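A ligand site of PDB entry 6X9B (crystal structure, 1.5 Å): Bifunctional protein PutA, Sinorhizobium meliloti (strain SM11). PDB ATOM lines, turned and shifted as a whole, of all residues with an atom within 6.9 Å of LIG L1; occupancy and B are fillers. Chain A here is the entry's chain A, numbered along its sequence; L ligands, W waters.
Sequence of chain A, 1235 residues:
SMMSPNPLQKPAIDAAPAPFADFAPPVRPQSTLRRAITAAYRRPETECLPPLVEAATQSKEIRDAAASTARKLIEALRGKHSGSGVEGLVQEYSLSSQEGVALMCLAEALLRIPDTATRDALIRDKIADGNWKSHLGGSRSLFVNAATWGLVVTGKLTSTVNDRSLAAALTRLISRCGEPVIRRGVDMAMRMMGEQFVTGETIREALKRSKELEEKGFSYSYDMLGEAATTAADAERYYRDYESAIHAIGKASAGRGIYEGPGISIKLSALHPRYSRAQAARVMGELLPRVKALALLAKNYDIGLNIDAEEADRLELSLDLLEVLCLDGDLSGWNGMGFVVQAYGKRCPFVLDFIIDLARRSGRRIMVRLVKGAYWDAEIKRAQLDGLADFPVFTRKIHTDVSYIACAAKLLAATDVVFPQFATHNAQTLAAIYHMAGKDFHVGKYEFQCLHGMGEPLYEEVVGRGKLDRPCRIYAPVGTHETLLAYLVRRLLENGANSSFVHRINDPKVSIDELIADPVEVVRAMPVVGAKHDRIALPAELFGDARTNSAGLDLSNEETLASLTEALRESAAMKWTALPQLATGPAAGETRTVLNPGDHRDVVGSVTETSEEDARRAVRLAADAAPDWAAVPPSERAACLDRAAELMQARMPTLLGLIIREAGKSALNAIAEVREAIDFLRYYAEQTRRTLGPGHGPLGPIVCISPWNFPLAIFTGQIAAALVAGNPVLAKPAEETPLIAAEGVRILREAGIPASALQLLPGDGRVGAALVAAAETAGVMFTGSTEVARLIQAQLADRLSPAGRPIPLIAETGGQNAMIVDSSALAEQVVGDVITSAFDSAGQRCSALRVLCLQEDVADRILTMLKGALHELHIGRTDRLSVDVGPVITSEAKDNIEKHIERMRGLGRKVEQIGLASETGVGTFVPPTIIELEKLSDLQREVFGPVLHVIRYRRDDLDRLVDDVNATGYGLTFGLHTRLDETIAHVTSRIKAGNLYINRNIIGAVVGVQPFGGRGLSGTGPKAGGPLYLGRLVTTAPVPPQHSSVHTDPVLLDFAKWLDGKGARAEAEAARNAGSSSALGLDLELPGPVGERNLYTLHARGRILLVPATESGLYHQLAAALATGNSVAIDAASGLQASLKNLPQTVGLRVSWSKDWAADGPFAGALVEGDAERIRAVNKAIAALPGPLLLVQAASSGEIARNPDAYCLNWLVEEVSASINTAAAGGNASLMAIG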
ATOM      1  N   GLU A 676      -0.944  -3.688  17.786  1.00  0.00           N
ATOM      2  CA  GLU A 676      -0.690  -2.607  16.834  1.00  0.00           C
ATOM      3  C   GLU A 676      -1.230  -2.944  15.453  1.00  0.00           C
ATOM      4  O   GLU A 676      -1.834  -2.101  14.788  1.00  0.00           O
ATOM      5  CB  GLU A 676       0.809  -2.294  16.768  1.00  0.00           C
ATOM      6  CG  GLU A 676       1.069  -0.929  16.148  1.00  0.00           C
ATOM      7  CD  GLU A 676       2.511  -0.474  16.242  1.00  0.00           C
ATOM      8  OE1 GLU A 676       3.316  -1.156  16.916  1.00  0.00           O
ATOM      9  OE2 GLU A 676       2.830   0.573  15.640  1.00  0.00           O
ATOM     10  N   PHE A 680      -3.960  -0.788  13.487  1.00  0.00           N
ATOM     11  CA  PHE A 680      -3.804  -0.259  12.126  1.00  0.00           C
ATOM     12  C   PHE A 680      -5.007  -0.611  11.258  1.00  0.00           C
ATOM     13  O   PHE A 680      -5.564   0.239  10.559  1.00  0.00           O
ATOM     14  CB  PHE A 680      -2.551  -0.834  11.450  1.00  0.00           C
ATOM     15  CG  PHE A 680      -1.280  -0.109  11.803  1.00  0.00           C
ATOM     16  CD1 PHE A 680      -1.165   1.278  11.665  1.00  0.00           C
ATOM     17  CD2 PHE A 680      -0.172  -0.821  12.258  1.00  0.00           C
ATOM     18  CE1 PHE A 680       0.006   1.940  11.985  1.00  0.00           C
ATOM     19  CE2 PHE A 680       1.014  -0.175  12.576  1.00  0.00           C
ATOM     20  CZ  PHE A 680       1.118   1.199  12.452  1.00  0.00           C
ATOM     21  N   ASN A 709      11.756  -5.777  12.232  1.00  0.00           N
ATOM     22  CA  ASN A 709      11.629  -5.560  13.678  1.00  0.00           C
ATOM     23  C   ASN A 709      10.209  -5.349  14.140  1.00  0.00           C
ATOM     24  O   ASN A 709       9.932  -5.481  15.341  1.00  0.00           O
ATOM     25  CB  ASN A 709      12.525  -4.407  14.147  1.00  0.00           C
ATOM     26  CG  ASN A 709      12.074  -3.068  13.639  1.00  0.00           C
ATOM     27  OD1 ASN A 709      11.762  -2.909  12.456  1.00  0.00           O
ATOM     28  ND2 ASN A 709      12.060  -2.078  14.521  1.00  0.00           N
ATOM     29  N   PHE A 710       9.294  -5.024  13.238  1.00  0.00           N
ATOM     30  CA  PHE A 710       7.855  -5.106  13.485  1.00  0.00           C
ATOM     31  C   PHE A 710       7.265  -5.905  12.342  1.00  0.00           C
ATOM     32  O   PHE A 710       6.582  -5.366  11.467  1.00  0.00           O
ATOM     33  CB  PHE A 710       7.215  -3.735  13.676  1.00  0.00           C
ATOM     34  CG  PHE A 710       7.605  -3.125  14.978  1.00  0.00           C
ATOM     35  CD1 PHE A 710       6.931  -3.455  16.135  1.00  0.00           C
ATOM     36  CD2 PHE A 710       8.723  -2.307  15.073  1.00  0.00           C
ATOM     37  CE1 PHE A 710       7.323  -2.927  17.361  1.00  0.00           C
ATOM     38  CE2 PHE A 710       9.119  -1.779  16.283  1.00  0.00           C
ATOM     39  CZ  PHE A 710       8.411  -2.097  17.430  1.00  0.00           C
ATOM     40  N   ALA A 713       3.254  -5.796  12.566  1.00  0.00           N
ATOM     41  CA  ALA A 713       2.528  -4.545  12.731  1.00  0.00           C
ATOM     42  C   ALA A 713       2.804  -3.573  11.587  1.00  0.00           C
ATOM     43  O   ALA A 713       1.878  -3.084  10.932  1.00  0.00           O
ATOM     44  CB  ALA A 713       2.853  -3.910  14.075  1.00  0.00           C
ATOM     45  N   ILE A 714       4.078  -3.239  11.359  1.00  0.00           N
ATOM     46  CA  ILE A 714       4.393  -2.302  10.285  1.00  0.00           C
ATOM     47  C   ILE A 714       4.111  -2.923   8.918  1.00  0.00           C
ATOM     48  O   ILE A 714       3.631  -2.245   7.996  1.00  0.00           O
ATOM     49  CB  ILE A 714       5.848  -1.787  10.404  1.00  0.00           C
ATOM     50  CG1 ILE A 714       5.996  -0.928  11.660  1.00  0.00           C
ATOM     51  CG2 ILE A 714       6.286  -1.065   9.126  1.00  0.00           C
ATOM     52  CD1 ILE A 714       7.428  -0.565  11.987  1.00  0.00           C
ATOM     53  N   ARG A 845      13.834  -1.473  18.445  1.00  0.00           N
ATOM     54  CA  ARG A 845      12.739  -0.616  18.038  1.00  0.00           C
ATOM     55  C   ARG A 845      13.354   0.606  17.377  1.00  0.00           C
ATOM     56  O   ARG A 845      14.388   1.103  17.816  1.00  0.00           O
ATOM     57  CB  ARG A 845      11.962  -0.147  19.273  1.00  0.00           C
ATOM     58  CG  ARG A 845      11.130  -1.224  19.937  1.00  0.00           C
ATOM     59  CD  ARG A 845      10.334  -0.629  21.083  1.00  0.00           C
ATOM     60  NE  ARG A 845       9.602  -1.634  21.854  1.00  0.00           N
ATOM     61  CZ  ARG A 845       8.290  -1.873  21.762  1.00  0.00           C
ATOM     62  NH1 ARG A 845       7.527  -1.170  20.920  1.00  0.00           N
ATOM     63  NH2 ARG A 845       7.740  -2.814  22.512  1.00  0.00           N
ATOM     64  N   CYS A 846      12.718   1.082  16.296  1.00  0.00           N
ATOM     65  CA  CYS A 846      13.195   2.332  15.722  1.00  0.00           C
ATOM     66  C   CYS A 846      13.028   3.484  16.712  1.00  0.00           C
ATOM     67  O   CYS A 846      13.801   4.453  16.670  1.00  0.00           O
ATOM     68  CB  CYS A 846      12.475   2.649  14.413  1.00  0.00           C
ATOM     69  SG  CYS A 846      10.697   2.583  14.536  1.00  0.00           S
ATOM     70  N   SER A 847      12.062   3.374  17.624  1.00  0.00           N
ATOM     71  CA  SER A 847      11.792   4.365  18.671  1.00  0.00           C
ATOM     72  C   SER A 847      12.715   4.238  19.882  1.00  0.00           C
ATOM     73  O   SER A 847      12.595   5.047  20.807  1.00  0.00           O
ATOM     74  CB  SER A 847      10.346   4.231  19.142  1.00  0.00           C
ATOM     75  OG  SER A 847      10.078   2.882  19.514  1.00  0.00           O
ATOM     76  N   ALA A 848      13.638   3.280  19.882  1.00  0.00           N
ATOM     77  CA  ALA A 848      14.378   2.964  21.100  1.00  0.00           C
ATOM     78  C   ALA A 848      15.280   4.116  21.529  1.00  0.00           C
ATOM     79  O   ALA A 848      15.765   4.895  20.709  1.00  0.00           O
ATOM     80  CB  ALA A 848      15.221   1.702  20.891  1.00  0.00           C
ATOM     81  N   LEU A 972      13.167  11.326  15.273  1.00  0.00           N
ATOM     82  CA  LEU A 972      12.113  10.330  15.368  1.00  0.00           C
ATOM     83  C   LEU A 972      11.404  10.432  16.718  1.00  0.00           C
ATOM     84  O   LEU A 972      10.373  11.116  16.821  1.00  0.00           O
ATOM     85  CB  LEU A 972      12.662   8.941  15.064  1.00  0.00           C
ATOM     86  CG  LEU A 972      11.648   7.807  14.983  1.00  0.00           C
ATOM     87  CD1 LEU A 972      10.522   8.177  14.039  1.00  0.00           C
ATOM     88  CD2 LEU A 972      12.356   6.576  14.458  1.00  0.00           C
ATOM     89  N   THR A 973      11.913   9.778  17.764  1.00  0.00           N
ATOM     90  CA  THR A 973      11.342   9.925  19.092  1.00  0.00           C
ATOM     91  C   THR A 973      12.263  10.733  19.991  1.00  0.00           C
ATOM     92  O   THR A 973      13.478  10.803  19.778  1.00  0.00           O
ATOM     93  CB  THR A 973      11.055   8.566  19.753  1.00  0.00           C
ATOM     94  OG1 THR A 973      12.269   7.836  19.877  1.00  0.00           O
ATOM     95  CG2 THR A 973      10.062   7.774  18.918  1.00  0.00           C
ATOM     96  N   TYR A 997       7.734  12.566  24.142  1.00  0.00           N
ATOM     97  CA  TYR A 997       7.220  11.844  25.301  1.00  0.00           C
ATOM     98  C   TYR A 997       7.686  12.560  26.566  1.00  0.00           C
ATOM     99  O   TYR A 997       8.887  12.762  26.761  1.00  0.00           O
ATOM    100  CB  TYR A 997       7.713  10.391  25.285  1.00  0.00           C
ATOM    101  CG  TYR A 997       7.200   9.613  24.082  1.00  0.00           C
ATOM    102  CD1 TYR A 997       5.914   9.064  24.090  1.00  0.00           C
ATOM    103  CD2 TYR A 997       7.978   9.455  22.948  1.00  0.00           C
ATOM    104  CE1 TYR A 997       5.436   8.344  22.990  1.00  0.00           C
ATOM    105  CE2 TYR A 997       7.507   8.722  21.850  1.00  0.00           C
ATOM    106  CZ  TYR A 997       6.236   8.185  21.881  1.00  0.00           C
ATOM    107  OH  TYR A 997       5.757   7.489  20.783  1.00  0.00           O
ATOM    108  N   ILE A1002       9.667   6.212  25.757  1.00  0.00           N
ATOM    109  CA  ILE A1002       9.577   6.761  24.403  1.00  0.00           C
ATOM    110  C   ILE A1002       9.208   5.702  23.377  1.00  0.00           C
ATOM    111  O   ILE A1002       9.360   5.933  22.168  1.00  0.00           O
ATOM    112  CB  ILE A1002      10.832   7.557  23.994  1.00  0.00           C
ATOM    113  CG1 ILE A1002      12.038   6.646  23.762  1.00  0.00           C
ATOM    114  CG2 ILE A1002      11.163   8.606  25.050  1.00  0.00           C
ATOM    115  CD1 ILE A1002      13.271   7.381  23.230  1.00  0.00           C
ATOM    116  N   ILE A1003       8.708   4.554  23.823  1.00  0.00           N
ATOM    117  CA  ILE A1003       8.462   3.435  22.929  1.00  0.00           C
ATOM    118  C   ILE A1003       6.978   3.065  22.923  1.00  0.00           C
ATOM    119  O   ILE A1003       6.191   3.481  23.779  1.00  0.00           O
ATOM    120  CB  ILE A1003       9.329   2.214  23.278  1.00  0.00           C
ATOM    121  CG1 ILE A1003       9.029   1.732  24.696  1.00  0.00           C
ATOM    122  CG2 ILE A1003      10.793   2.520  23.057  1.00  0.00           C
ATOM    123  CD1 ILE A1003       9.583   0.325  24.966  1.00  0.00           C
ATOM    124  N   GLY A1004       6.610   2.252  21.954  1.00  0.00           N
ATOM    125  CA  GLY A1004       5.271   1.710  21.941  1.00  0.00           C
ATOM    126  C   GLY A1004       4.203   2.707  21.537  1.00  0.00           C
ATOM    127  O   GLY A1004       3.101   2.670  22.086  1.00  0.00           O
ATOM    128  N   ALA A1005       4.500   3.573  20.575  1.00  0.00           N
ATOM    129  CA  ALA A1005       3.509   4.504  20.063  1.00  0.00           C
ATOM    130  C   ALA A1005       2.249   3.754  19.652  1.00  0.00           C
ATOM    131  O   ALA A1005       2.304   2.701  19.007  1.00  0.00           O
ATOM    132  CB  ALA A1005       4.058   5.274  18.857  1.00  0.00           C
ATOM    133  N   VAL A1006       1.107   4.308  20.034  1.00  0.00           N
ATOM    134  CA  VAL A1006      -0.197   3.682  19.834  1.00  0.00           C
ATOM    135  C   VAL A1006      -0.894   4.333  18.653  1.00  0.00           C
ATOM    136  O   VAL A1006      -1.037   5.553  18.598  1.00  0.00           O
ATOM    137  CB  VAL A1006      -1.053   3.820  21.106  1.00  0.00           C
ATOM    138  CG1 VAL A1006      -2.468   3.311  20.854  1.00  0.00           C
ATOM    139  CG2 VAL A1006      -0.370   3.075  22.265  1.00  0.00           C
ATOM    140  N   GLN A1010      -0.691   8.163  19.597  1.00  0.00           N
ATOM    141  CA  GLN A1010       0.553   8.803  19.184  1.00  0.00           C
ATOM    142  C   GLN A1010       0.826   8.391  17.728  1.00  0.00           C
ATOM    143  O   GLN A1010       1.583   7.444  17.469  1.00  0.00           O
ATOM    144  CB  GLN A1010       1.725   8.465  20.095  1.00  0.00           C
ATOM    145  CG  GLN A1010       1.458   8.720  21.586  1.00  0.00           C
ATOM    146  CD  GLN A1010       1.017   7.463  22.333  1.00  0.00           C
ATOM    147  OE1 GLN A1010       1.370   6.346  21.955  1.00  0.00           O
ATOM    148  NE2 GLN A1010       0.250   7.654  23.405  1.00  0.00           N
ATOM    149  N   PHE A1012       2.683   7.960  14.561  1.00  0.00           N
ATOM    150  CA  PHE A1012       4.109   7.707  14.672  1.00  0.00           C
ATOM    151  C   PHE A1012       4.844   8.065  13.385  1.00  0.00           C
ATOM    152  O   PHE A1012       4.435   7.674  12.282  1.00  0.00           O
ATOM    153  CB  PHE A1012       4.392   6.265  15.083  1.00  0.00           C
ATOM    154  CG  PHE A1012       5.844   5.994  15.327  1.00  0.00           C
ATOM    155  CD1 PHE A1012       6.438   6.366  16.527  1.00  0.00           C
ATOM    156  CD2 PHE A1012       6.625   5.379  14.357  1.00  0.00           C
ATOM    157  CE1 PHE A1012       7.770   6.137  16.750  1.00  0.00           C
ATOM    158  CE2 PHE A1012       7.965   5.146  14.576  1.00  0.00           C
ATOM    159  CZ  PHE A1012       8.549   5.513  15.784  1.00  0.00           C
ATOM    160  N   GLY A1013       5.946   8.789  13.536  1.00  0.00           N
ATOM    161  CA  GLY A1013       6.787   9.087  12.392  1.00  0.00           C
ATOM    162  C   GLY A1013       7.586  10.343  12.615  1.00  0.00           C
ATOM    163  O   GLY A1013       7.095  11.294  13.244  1.00  0.00           O
HETATM  164  N1  LIG L   1       5.834   0.186  16.994  1.00  0.00           N
HETATM  165  C1  LIG L   1       5.714   1.544  17.617  1.00  0.00           C
HETATM  166  C2  LIG L   1       6.930   1.779  18.549  1.00  0.00           C
HETATM  167  O1  LIG L   1       7.685   0.814  18.764  1.00  0.00           O
HETATM  168  C3  LIG L   1       5.701   2.577  16.475  1.00  0.00           C
HETATM  169  C4  LIG L   1       6.499   1.857  15.377  1.00  0.00           C
HETATM  170  C5  LIG L   1       6.092   0.378  15.555  1.00  0.00           C
HETATM  171  O2  LIG L   1       7.850   2.034  15.591  1.00  0.00           O
HETATM  172  O3  LIG L   1       7.046   2.951  19.009  1.00  0.00           O
HETATM  173  P1  LG2 L   2      16.588  -2.491   6.041  1.00  0.00           P
HETATM  174  O1  LG2 L   2      16.880  -1.155   5.441  1.00  0.00           O
HETATM  175  O2  LG2 L   2      17.842  -3.311   6.184  1.00  0.00           O
HETATM  176  O3  LG2 L   2      15.492  -3.396   5.187  1.00  0.00           O
HETATM  177  C1  LG2 L   2      14.119  -3.032   5.195  1.00  0.00           C
HETATM  178  C2  LG2 L   2      13.467  -3.693   3.932  1.00  0.00           C
HETATM  179  O4  LG2 L   2      14.198  -3.100   2.620  1.00  0.00           O
HETATM  180  C3  LG2 L   2      13.625  -4.999   3.890  1.00  0.00           C
HETATM  181  O5  LG2 L   2      12.349  -5.627   3.402  1.00  0.00           O
HETATM  182  C4  LG2 L   2      14.775  -5.254   2.875  1.00  0.00           C
HETATM  183  O6  LG2 L   2      14.710  -6.514   2.322  1.00  0.00           O
HETATM  184  C5  LG2 L   2      14.540  -4.122   1.852  1.00  0.00           C
HETATM  185  N1  LG2 L   2      15.748  -3.775   1.104  1.00  0.00           N
HETATM  186  C6  LG2 L   2      17.069  -3.851   1.283  1.00  0.00           C
HETATM  187  N2  LG2 L   2      17.644  -3.306   0.200  1.00  0.00           N
HETATM  188  C7  LG2 L   2      16.682  -2.895  -0.651  1.00  0.00           C
HETATM  189  C8  LG2 L   2      16.760  -2.275  -1.904  1.00  0.00           C
HETATM  190  N3  LG2 L   2      18.082  -1.968  -2.511  1.00  0.00           N
HETATM  191  N4  LG2 L   2      15.658  -1.955  -2.554  1.00  0.00           N
HETATM  192  C9  LG2 L   2      14.421  -2.242  -1.986  1.00  0.00           C
HETATM  193  N5  LG2 L   2      14.333  -2.848  -0.772  1.00  0.00           N
HETATM  194  C10 LG2 L   2      15.492  -3.172  -0.093  1.00  0.00           C
HETATM  195  O7  LG2 L   2      15.891  -2.214   7.489  1.00  0.00           O
HETATM  196  P2  LG2 L   2      15.629  -3.379   8.669  1.00  0.00           P
HETATM  197  O8  LG2 L   2      17.025  -3.901   9.088  1.00  0.00           O
HETATM  198  O9  LG2 L   2      14.727  -4.479   8.188  1.00  0.00           O
HETATM  199  O10 LG2 L   2      14.946  -2.573   9.920  1.00  0.00           O
HETATM  200  C11 LG2 L   2      15.762  -1.774  10.775  1.00  0.00           C
HETATM  201  C12 LG2 L   2      15.777  -0.307  10.352  1.00  0.00           C
HETATM  202  O11 LG2 L   2      14.271   0.159  10.084  1.00  0.00           O
HETATM  203  C13 LG2 L   2      16.251   0.484  11.316  1.00  0.00           C
HETATM  204  O12 LG2 L   2      17.181   1.525  10.697  1.00  0.00           O
HETATM  205  C14 LG2 L   2      15.054   1.119  11.951  1.00  0.00           C
HETATM  206  O13 LG2 L   2      15.302   2.341  12.587  1.00  0.00           O
HETATM  207  C15 LG2 L   2      14.155   1.278  10.683  1.00  0.00           C
HETATM  208  N6  LG2 L   2      12.753   1.400  11.140  1.00  0.00           N
HETATM  209  C16 LG2 L   2      12.103   2.615  11.054  1.00  0.00           C
HETATM  210  C17 LG2 L   2      10.804   2.666  11.519  1.00  0.00           C
HETATM  211  C18 LG2 L   2      10.001   4.008  11.442  1.00  0.00           C
HETATM  212  O14 LG2 L   2       8.819   3.972  11.642  1.00  0.00           O
HETATM  213  N7  LG2 L   2      10.720   5.269  11.146  1.00  0.00           N
HETATM  214  C19 LG2 L   2      10.184   1.535  11.996  1.00  0.00           C
HETATM  215  C20 LG2 L   2      10.864   0.343  12.128  1.00  0.00           C
HETATM  216  C21 LG2 L   2      12.168   0.295  11.671  1.00  0.00           C
HETATM  217  O   HOH W   1       9.843   1.122  17.164  1.00  0.00           O
HETATM  218  O   HOH W   2       7.462   5.621  20.166  1.00  0.00           O
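Merely in contact with LIG L1: Phe 710 (3.3 Å), Ile 714 (3.9 Å), Ile 1003 (3.9 Å) and Phe 1012 (3.3 Å).
Hydrophobic or aromatic side chains that line LIG L1: Phe 710, Ile 714, Ala 1005 and Phe 1012.
Ten residues have an atom within 4 Å of LIG L1: Glu 676, Phe 710, Ile 714, Arg 845, Cys 846, Ser 847, Ile 1003, Gly 1004, Ala 1005 and Phe 1012.
The backbone carbonyl oxygen (O) of Ser 847 sits at hydrogen-bond distance from the side-chain hydroxyl (OG1) of Thr 973 (3.0 Å).
Water W1 lies within hydrogen-bond range of O2 of LIG L1 (2.7 Å), OG of Ser 847 (2.9 Å) and N of Cys 846 (3.0 Å).
Water W2 lies within hydrogen-bond range of the side-chain hydroxyl (OH) of Tyr 997 (2.6 Å), the backbone carbonyl oxygen (O) of Ile 1002 (2.8 Å) and an oxygen (O3) of LIG L1 (2.9 Å).
The side-chain carboxylate (OE1) of Glu 676 is in salt-bridge range of a nitrogen (N1) of LIG L1 (2.9 Å).
The guanidinium group (NH1) of Arg 845 lies within salt-bridge range of an oxygen (O1) of LIG L1 (2.9 Å).
The backbone NH (N) of Ala 1005 is in hydrogen-bond range of an oxygen (O3) of LIG L1, 3.1 Å away.
An oxygen (O3) of LIG L1 sits at hydrogen-bond distance from the backbone NH (N) of Gly 1004.
The side-chain hydroxyl (OG) of Ser 847 sits at hydrogen-bond distance from an oxygen (O3) of LIG L1 (3.1 Å).
An oxygen (O2) of LIG L1 is in hydrogen-bond range of the side-chain sulfur of Cys 846 (3.1 Å).
An oxygen (O14) of LG2 L2 lies close to the side-chain sulfur of Cys 846, 3.7 Å away.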
